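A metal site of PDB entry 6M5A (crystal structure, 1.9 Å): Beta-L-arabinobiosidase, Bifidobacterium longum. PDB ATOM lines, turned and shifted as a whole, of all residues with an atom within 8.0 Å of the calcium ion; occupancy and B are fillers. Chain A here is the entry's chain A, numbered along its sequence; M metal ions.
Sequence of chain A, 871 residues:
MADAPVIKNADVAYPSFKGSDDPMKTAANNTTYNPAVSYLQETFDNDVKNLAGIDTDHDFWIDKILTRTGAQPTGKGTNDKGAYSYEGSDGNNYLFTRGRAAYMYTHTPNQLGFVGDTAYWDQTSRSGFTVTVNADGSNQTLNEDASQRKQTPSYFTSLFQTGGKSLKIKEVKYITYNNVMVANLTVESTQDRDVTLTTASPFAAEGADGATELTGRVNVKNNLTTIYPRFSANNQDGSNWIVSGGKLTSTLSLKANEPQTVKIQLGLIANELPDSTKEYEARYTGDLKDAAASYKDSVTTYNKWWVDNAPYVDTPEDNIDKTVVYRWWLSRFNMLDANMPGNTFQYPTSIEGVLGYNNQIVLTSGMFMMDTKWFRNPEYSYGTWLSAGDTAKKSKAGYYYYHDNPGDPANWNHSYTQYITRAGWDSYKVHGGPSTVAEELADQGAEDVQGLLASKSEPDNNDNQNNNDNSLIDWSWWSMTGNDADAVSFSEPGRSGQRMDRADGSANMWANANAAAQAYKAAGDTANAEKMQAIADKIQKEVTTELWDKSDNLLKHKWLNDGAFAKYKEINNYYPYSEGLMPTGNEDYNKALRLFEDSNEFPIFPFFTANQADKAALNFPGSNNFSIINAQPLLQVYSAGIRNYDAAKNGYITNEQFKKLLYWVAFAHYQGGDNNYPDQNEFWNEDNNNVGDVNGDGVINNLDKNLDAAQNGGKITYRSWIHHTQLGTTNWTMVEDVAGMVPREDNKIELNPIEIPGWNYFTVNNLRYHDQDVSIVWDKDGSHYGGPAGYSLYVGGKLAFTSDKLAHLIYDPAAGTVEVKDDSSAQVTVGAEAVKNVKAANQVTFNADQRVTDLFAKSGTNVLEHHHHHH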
ATOM      1  N   LEU A 452      15.200  33.347   4.276  1.00  0.00           N
ATOM      2  CA  LEU A 452      14.347  33.107   3.087  1.00  0.00           C
ATOM      3  C   LEU A 452      14.837  31.856   2.353  1.00  0.00           C
ATOM      4  O   LEU A 452      13.970  31.018   1.952  1.00  0.00           O
ATOM      5  CB  LEU A 452      14.353  34.326   2.173  1.00  0.00           C
ATOM      6  CG  LEU A 452      13.735  35.602   2.730  1.00  0.00           C
ATOM      7  CD1 LEU A 452      13.364  36.557   1.598  1.00  0.00           C
ATOM      8  CD2 LEU A 452      12.545  35.327   3.594  1.00  0.00           C
ATOM      9  N   LEU A 453      16.153  31.691   2.183  1.00  0.00           N
ATOM     10  CA  LEU A 453      16.680  30.530   1.440  1.00  0.00           C
ATOM     11  C   LEU A 453      16.237  29.242   2.159  1.00  0.00           C
ATOM     12  O   LEU A 453      15.967  28.251   1.480  1.00  0.00           O
ATOM     13  CB  LEU A 453      18.201  30.634   1.308  1.00  0.00           C
ATOM     14  CG  LEU A 453      18.714  31.555   0.208  1.00  0.00           C
ATOM     15  CD1 LEU A 453      20.194  31.776   0.347  1.00  0.00           C
ATOM     16  CD2 LEU A 453      18.361  31.033  -1.192  1.00  0.00           C
ATOM     17  N   ASN A 464       6.921  30.462   4.020  1.00  0.00           N
ATOM     18  CA  ASN A 464       7.694  29.514   3.168  1.00  0.00           C
ATOM     19  C   ASN A 464       7.839  30.108   1.778  1.00  0.00           C
ATOM     20  O   ASN A 464       6.862  30.109   0.990  1.00  0.00           O
ATOM     21  CB  ASN A 464       7.032  28.130   3.210  1.00  0.00           C
ATOM     22  CG  ASN A 464       7.749  27.087   2.388  1.00  0.00           C
ATOM     23  OD1 ASN A 464       8.648  27.389   1.616  1.00  0.00           O
ATOM     24  ND2 ASN A 464       7.340  25.838   2.548  1.00  0.00           N
ATOM     25  N   GLN A 465       9.034  30.598   1.462  1.00  0.00           N
ATOM     26  CA  GLN A 465       9.311  31.303   0.196  1.00  0.00           C
ATOM     27  C   GLN A 465      10.312  30.454  -0.598  1.00  0.00           C
ATOM     28  O   GLN A 465      10.872  30.959  -1.609  1.00  0.00           O
ATOM     29  CB  GLN A 465       9.804  32.722   0.455  1.00  0.00           C
ATOM     30  CG  GLN A 465       8.808  33.611   1.208  1.00  0.00           C
ATOM     31  CD  GLN A 465       9.257  35.056   1.103  1.00  0.00           C
ATOM     32  OE1 GLN A 465       9.436  35.604   0.020  1.00  0.00           O
ATOM     33  NE2 GLN A 465       9.530  35.651   2.251  1.00  0.00           N
ATOM     34  N   ASN A 466      10.494  29.199  -0.251  1.00  0.00           N
ATOM     35  CA  ASN A 466      11.470  28.378  -0.992  1.00  0.00           C
ATOM     36  C   ASN A 466      11.140  26.890  -0.870  1.00  0.00           C
ATOM     37  O   ASN A 466      11.972  26.125  -0.350  1.00  0.00           O
ATOM     38  CB  ASN A 466      12.922  28.666  -0.588  1.00  0.00           C
ATOM     39  CG  ASN A 466      13.904  28.088  -1.582  1.00  0.00           C
ATOM     40  OD1 ASN A 466      13.536  27.770  -2.720  1.00  0.00           O
ATOM     41  ND2 ASN A 466      15.142  27.955  -1.157  1.00  0.00           N
ATOM     42  N   ASN A 467       9.963  26.487  -1.338  1.00  0.00           N
ATOM     43  CA  ASN A 467       9.459  25.126  -1.086  1.00  0.00           C
ATOM     44  C   ASN A 467      10.154  24.089  -1.988  1.00  0.00           C
ATOM     45  O   ASN A 467      10.077  22.896  -1.636  1.00  0.00           O
ATOM     46  CB  ASN A 467       7.943  25.031  -1.235  1.00  0.00           C
ATOM     47  CG  ASN A 467       7.374  23.871  -0.453  1.00  0.00           C
ATOM     48  OD1 ASN A 467       7.800  23.610   0.661  1.00  0.00           O
ATOM     49  ND2 ASN A 467       6.383  23.193  -1.014  1.00  0.00           N
ATOM     50  N   ASN A 468      10.878  24.481  -3.050  1.00  0.00           N
ATOM     51  CA  ASN A 468      11.716  23.505  -3.802  1.00  0.00           C
ATOM     52  C   ASN A 468      13.180  23.595  -3.343  1.00  0.00           C
ATOM     53  O   ASN A 468      13.997  22.918  -3.950  1.00  0.00           O
ATOM     54  CB  ASN A 468      11.558  23.571  -5.319  1.00  0.00           C
ATOM     55  CG  ASN A 468      11.948  24.913  -5.869  1.00  0.00           C
ATOM     56  OD1 ASN A 468      12.205  25.805  -5.092  1.00  0.00           O
ATOM     57  ND2 ASN A 468      11.922  25.084  -7.180  1.00  0.00           N
ATOM     58  N   ASP A 469      13.478  24.384  -2.318  1.00  0.00           N
ATOM     59  CA  ASP A 469      14.814  24.477  -1.678  1.00  0.00           C
ATOM     60  C   ASP A 469      15.933  24.748  -2.692  1.00  0.00           C
ATOM     61  O   ASP A 469      17.000  24.103  -2.623  1.00  0.00           O
ATOM     62  CB  ASP A 469      15.132  23.207  -0.877  1.00  0.00           C
ATOM     63  CG  ASP A 469      16.175  23.450   0.198  1.00  0.00           C
ATOM     64  OD1 ASP A 469      16.475  24.644   0.473  1.00  0.00           O
ATOM     65  OD2 ASP A 469      16.687  22.444   0.774  1.00  0.00           O
ATOM     66  N   ASN A 470      15.721  25.633  -3.673  1.00  0.00           N
ATOM     67  CA  ASN A 470      16.805  26.025  -4.616  1.00  0.00           C
ATOM     68  C   ASN A 470      17.241  27.440  -4.225  1.00  0.00           C
ATOM     69  O   ASN A 470      17.050  27.843  -3.054  1.00  0.00           O
ATOM     70  CB  ASN A 470      16.406  25.868  -6.091  1.00  0.00           C
ATOM     71  CG  ASN A 470      15.272  26.778  -6.503  1.00  0.00           C
ATOM     72  OD1 ASN A 470      14.727  27.545  -5.688  1.00  0.00           O
ATOM     73  ND2 ASN A 470      14.889  26.718  -7.771  1.00  0.00           N
ATOM     74  N   SER A 471      17.755  28.228  -5.145  1.00  0.00           N
ATOM     75  CA  SER A 471      18.226  29.596  -4.804  1.00  0.00           C
ATOM     76  C   SER A 471      17.270  30.633  -5.407  1.00  0.00           C
ATOM     77  O   SER A 471      17.666  31.771  -5.600  1.00  0.00           O
ATOM     78  CB  SER A 471      19.662  29.782  -5.217  1.00  0.00           C
ATOM     79  OG  SER A 471      20.472  28.841  -4.558  1.00  0.00           O
ATOM     80  N   LEU A 472      16.036  30.245  -5.665  1.00  0.00           N
ATOM     81  CA  LEU A 472      14.997  31.148  -6.194  1.00  0.00           C
ATOM     82  C   LEU A 472      13.884  31.221  -5.160  1.00  0.00           C
ATOM     83  O   LEU A 472      13.485  30.209  -4.604  1.00  0.00           O
ATOM     84  CB  LEU A 472      14.494  30.611  -7.520  1.00  0.00           C
ATOM     85  CG  LEU A 472      15.512  30.538  -8.649  1.00  0.00           C
ATOM     86  CD1 LEU A 472      14.817  30.053  -9.918  1.00  0.00           C
ATOM     87  CD2 LEU A 472      16.173  31.891  -8.900  1.00  0.00           C
ATOM     88  N   ILE A 473      13.383  32.407  -4.917  1.00  0.00           N
ATOM     89  CA  ILE A 473      12.130  32.586  -4.140  1.00  0.00           C
ATOM     90  C   ILE A 473      10.952  32.017  -4.931  1.00  0.00           C
ATOM     91  O   ILE A 473      10.816  32.348  -6.119  1.00  0.00           O
ATOM     92  CB  ILE A 473      11.919  34.071  -3.827  1.00  0.00           C
ATOM     93  CG1 ILE A 473      12.979  34.522  -2.828  1.00  0.00           C
ATOM     94  CG2 ILE A 473      10.522  34.270  -3.302  1.00  0.00           C
ATOM     95  CD1 ILE A 473      12.720  33.959  -1.416  1.00  0.00           C
ATOM     96  N   ASP A 474      10.088  31.263  -4.247  1.00  0.00           N
ATOM     97  CA  ASP A 474       8.802  30.794  -4.807  1.00  0.00           C
ATOM     98  C   ASP A 474       7.674  31.190  -3.853  1.00  0.00           C
ATOM     99  O   ASP A 474       7.872  31.202  -2.631  1.00  0.00           O
ATOM    100  CB  ASP A 474       8.839  29.306  -5.145  1.00  0.00           C
ATOM    101  CG  ASP A 474       9.292  28.413  -4.014  1.00  0.00           C
ATOM    102  OD1 ASP A 474       8.455  28.043  -3.164  1.00  0.00           O
ATOM    103  OD2 ASP A 474      10.473  28.049  -3.998  1.00  0.00           O
ATOM    104  N   TRP A 475       6.537  31.500  -4.446  1.00  0.00           N
ATOM    105  CA  TRP A 475       5.259  31.860  -3.790  1.00  0.00           C
ATOM    106  C   TRP A 475       4.120  31.154  -4.501  1.00  0.00           C
ATOM    107  O   TRP A 475       4.248  30.840  -5.712  1.00  0.00           O
ATOM    108  CB  TRP A 475       4.942  33.364  -3.870  1.00  0.00           C
ATOM    109  CG  TRP A 475       5.987  34.264  -3.374  1.00  0.00           C
ATOM    110  CD1 TRP A 475       6.814  34.093  -2.307  1.00  0.00           C
ATOM    111  CD2 TRP A 475       6.371  35.480  -4.004  1.00  0.00           C
ATOM    112  NE1 TRP A 475       7.677  35.154  -2.216  1.00  0.00           N
ATOM    113  CE2 TRP A 475       7.444  35.992  -3.261  1.00  0.00           C
ATOM    114  CE3 TRP A 475       5.884  36.183  -5.104  1.00  0.00           C
ATOM    115  CZ2 TRP A 475       8.043  37.201  -3.580  1.00  0.00           C
ATOM    116  CZ3 TRP A 475       6.497  37.360  -5.445  1.00  0.00           C
ATOM    117  CH2 TRP A 475       7.566  37.856  -4.696  1.00  0.00           C
ATOM    118  N   ARG A 499       2.722  26.939  -6.736  1.00  0.00           N
ATOM    119  CA  ARG A 499       3.922  27.760  -6.501  1.00  0.00           C
ATOM    120  C   ARG A 499       4.684  27.918  -7.806  1.00  0.00           C
ATOM    121  O   ARG A 499       4.786  26.941  -8.616  1.00  0.00           O
ATOM    122  CB  ARG A 499       4.828  27.155  -5.447  1.00  0.00           C
ATOM    123  CG  ARG A 499       4.366  27.412  -4.029  1.00  0.00           C
ATOM    124  CD  ARG A 499       5.317  26.743  -3.062  1.00  0.00           C
ATOM    125  NE  ARG A 499       4.893  27.090  -1.715  1.00  0.00           N
ATOM    126  CZ  ARG A 499       5.392  28.055  -0.952  1.00  0.00           C
ATOM    127  NH1 ARG A 499       4.850  28.289   0.226  1.00  0.00           N
ATOM    128  NH2 ARG A 499       6.431  28.769  -1.352  1.00  0.00           N
ATOM    129  N   MET A 500       5.311  29.076  -7.944  1.00  0.00           N
ATOM    130  CA  MET A 500       6.309  29.348  -8.987  1.00  0.00           C
ATOM    131  C   MET A 500       7.519  30.050  -8.370  1.00  0.00           C
ATOM    132  O   MET A 500       7.350  30.880  -7.492  1.00  0.00           O
ATOM    133  CB  MET A 500       5.716  30.186 -10.120  1.00  0.00           C
ATOM    134  CG  MET A 500       5.063  31.448  -9.637  1.00  0.00           C
ATOM    135  SD  MET A 500       4.569  32.450 -11.067  1.00  0.00           S
ATOM    136  CE  MET A 500       2.780  32.474 -10.931  1.00  0.00           C
ATOM    137  N   ASP A 501       8.710  29.673  -8.832  1.00  0.00           N
ATOM    138  CA  ASP A 501       9.970  30.417  -8.658  1.00  0.00           C
ATOM    139  C   ASP A 501       9.770  31.781  -9.338  1.00  0.00           C
ATOM    140  O   ASP A 501       9.367  31.829 -10.509  1.00  0.00           O
ATOM    141  CB  ASP A 501      11.169  29.595  -9.130  1.00  0.00           C
ATOM    142  CG  ASP A 501      11.710  28.594  -8.135  1.00  0.00           C
ATOM    143  OD1 ASP A 501      11.623  28.840  -6.907  1.00  0.00           O
ATOM    144  OD2 ASP A 501      12.255  27.564  -8.599  1.00  0.00           O
ATOM    145  N   ARG A 502       9.985  32.838  -8.591  1.00  0.00           N
ATOM    146  CA  ARG A 502       9.578  34.199  -8.945  1.00  0.00           C
ATOM    147  C   ARG A 502      10.773  35.029  -9.369  1.00  0.00           C
ATOM    148  O   ARG A 502      11.780  35.090  -8.650  1.00  0.00           O
ATOM    149  CB  ARG A 502       8.910  34.821  -7.720  1.00  0.00           C
ATOM    150  CG  ARG A 502       7.565  34.226  -7.377  1.00  0.00           C
ATOM    151  CD  ARG A 502       6.530  34.535  -8.422  1.00  0.00           C
ATOM    152  NE  ARG A 502       6.222  35.951  -8.539  1.00  0.00           N
ATOM    153  CZ  ARG A 502       5.279  36.425  -9.335  1.00  0.00           C
ATOM    154  NH1 ARG A 502       4.603  35.607 -10.129  1.00  0.00           N
ATOM    155  NH2 ARG A 502       5.033  37.728  -9.409  1.00  0.00           N
ATOM    156  N   SER A 506      13.023  36.681  -6.392  1.00  0.00           N
ATOM    157  CA  SER A 506      14.417  36.225  -6.553  1.00  0.00           C
ATOM    158  C   SER A 506      15.301  37.454  -6.781  1.00  0.00           C
ATOM    159  O   SER A 506      16.372  37.525  -6.171  1.00  0.00           O
ATOM    160  CB  SER A 506      14.551  35.149  -7.606  1.00  0.00           C
ATOM    161  OG  SER A 506      13.799  33.983  -7.247  1.00  0.00           O
ATOM    162  N   MET A 509      15.688  39.124  -3.389  1.00  0.00           N
ATOM    163  CA  MET A 509      16.579  38.374  -2.503  1.00  0.00           C
ATOM    164  C   MET A 509      18.005  38.567  -3.018  1.00  0.00           C
ATOM    165  O   MET A 509      18.864  38.728  -2.222  1.00  0.00           O
ATOM    166  CB  MET A 509      16.236  36.893  -2.452  1.00  0.00           C
ATOM    167  CG  MET A 509      17.137  36.117  -1.512  1.00  0.00           C
ATOM    168  SD  MET A 509      16.562  34.419  -1.385  1.00  0.00           S
ATOM    169  CE  MET A 509      16.678  33.880  -3.093  1.00  0.00           C
ATOM    170  N   GLU A 542      21.040  31.041 -10.991  1.00  0.00           N
ATOM    171  CA  GLU A 542      19.723  30.348 -11.122  1.00  0.00           C
ATOM    172  C   GLU A 542      18.692  31.245 -11.822  1.00  0.00           C
ATOM    173  O   GLU A 542      17.942  30.730 -12.653  1.00  0.00           O
ATOM    174  CB  GLU A 542      19.240  29.821  -9.780  1.00  0.00           C
ATOM    175  CG  GLU A 542      19.986  28.558  -9.380  1.00  0.00           C
ATOM    176  CD  GLU A 542      19.374  27.798  -8.210  1.00  0.00           C
ATOM    177  OE1 GLU A 542      18.198  28.058  -7.922  1.00  0.00           O
ATOM    178  OE2 GLU A 542      20.104  27.006  -7.551  1.00  0.00           O
ATOM    179  N   GLU A 546      17.411  29.566 -15.068  1.00  0.00           N
ATOM    180  CA  GLU A 546      16.100  28.908 -14.895  1.00  0.00           C
ATOM    181  C   GLU A 546      14.956  29.838 -15.279  1.00  0.00           C
ATOM    182  O   GLU A 546      13.942  29.322 -15.736  1.00  0.00           O
ATOM    183  CB  GLU A 546      15.921  28.411 -13.461  1.00  0.00           C
ATOM    184  CG  GLU A 546      16.975  27.385 -13.023  1.00  0.00           C
ATOM    185  CD  GLU A 546      16.676  26.745 -11.672  1.00  0.00           C
ATOM    186  OE1 GLU A 546      15.473  26.560 -11.347  1.00  0.00           O
ATOM    187  OE2 GLU A 546      17.629  26.467 -10.924  1.00  0.00           O
ATOM    188  N   LYS A 558       8.685  30.553 -13.141  1.00  0.00           N
ATOM    189  CA  LYS A 558       8.700  29.138 -13.518  1.00  0.00           C
ATOM    190  C   LYS A 558       7.928  28.327 -12.483  1.00  0.00           C
ATOM    191  O   LYS A 558       8.323  28.275 -11.312  1.00  0.00           O
ATOM    192  CB  LYS A 558      10.148  28.682 -13.642  1.00  0.00           C
ATOM    193  CG  LYS A 558      10.324  27.262 -14.121  1.00  0.00           C
ATOM    194  CD  LYS A 558      11.811  26.966 -14.318  1.00  0.00           C
ATOM    195  CE  LYS A 558      12.135  25.512 -14.497  1.00  0.00           C
ATOM    196  NZ  LYS A 558      13.454  25.351 -15.170  1.00  0.00           N
ATOM    197  N   LEU A 560       6.709  25.370 -10.241  1.00  0.00           N
ATOM    198  CA  LEU A 560       7.495  24.356  -9.508  1.00  0.00           C
ATOM    199  C   LEU A 560       7.088  22.957 -10.002  1.00  0.00           C
ATOM    200  O   LEU A 560       7.928  22.075 -10.096  1.00  0.00           O
ATOM    201  CB  LEU A 560       7.244  24.510  -8.006  1.00  0.00           C
ATOM    202  CG  LEU A 560       8.345  25.245  -7.231  1.00  0.00           C
ATOM    203  CD1 LEU A 560       8.620  26.578  -7.845  1.00  0.00           C
ATOM    204  CD2 LEU A 560       8.051  25.350  -5.750  1.00  0.00           C
HETATM  205 CA    CA M   1      12.567  28.134  -4.890  1.00  0.00          CA
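The backbone carbonyl oxygen (O) of Gln 465 lies within hydrogen-bond range of the backbone NH (N) of Asp 474 (2.8 Å).
The backbone NH of Asn 467 lies within hydrogen-bond range of the side-chain carboxylate of Asp 474 (2.8 Å).
The side-chain carboxylate of Asp 474 lies within salt-bridge range of the guanidinium group of Arg 499.
N of Asp 501 sits at hydrogen-bond distance from O of Lys 558 (2.9 Å).
OD1 of Asn 466 lies close to N of Asp 469, 3.4 Å away.
O of Leu 453 sits at hydrogen-bond distance from ND2 of Asn 466, at 2.8 Å.
The side-chain amide oxygen (OD1) of Asn 464 is in hydrogen-bond range of the backbone NH (N) of Asn 466 (3.2 Å).
Within 4 Å of the calcium ion: Asn 466, Asn 468, Asn 470, Leu 472, Asp 474 and Asp 501.
The calcium ion is bound by OD2 of Asp 474 (2.3 Å), O of Leu 472 (2.3 Å), OD1 of Asp 501 (2.3 Å), OD1 of Asn 468 (2.4 Å), OD1 of Asn 470 (2.4 Å) and OD1 of Asn 466 (2.4 Å).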
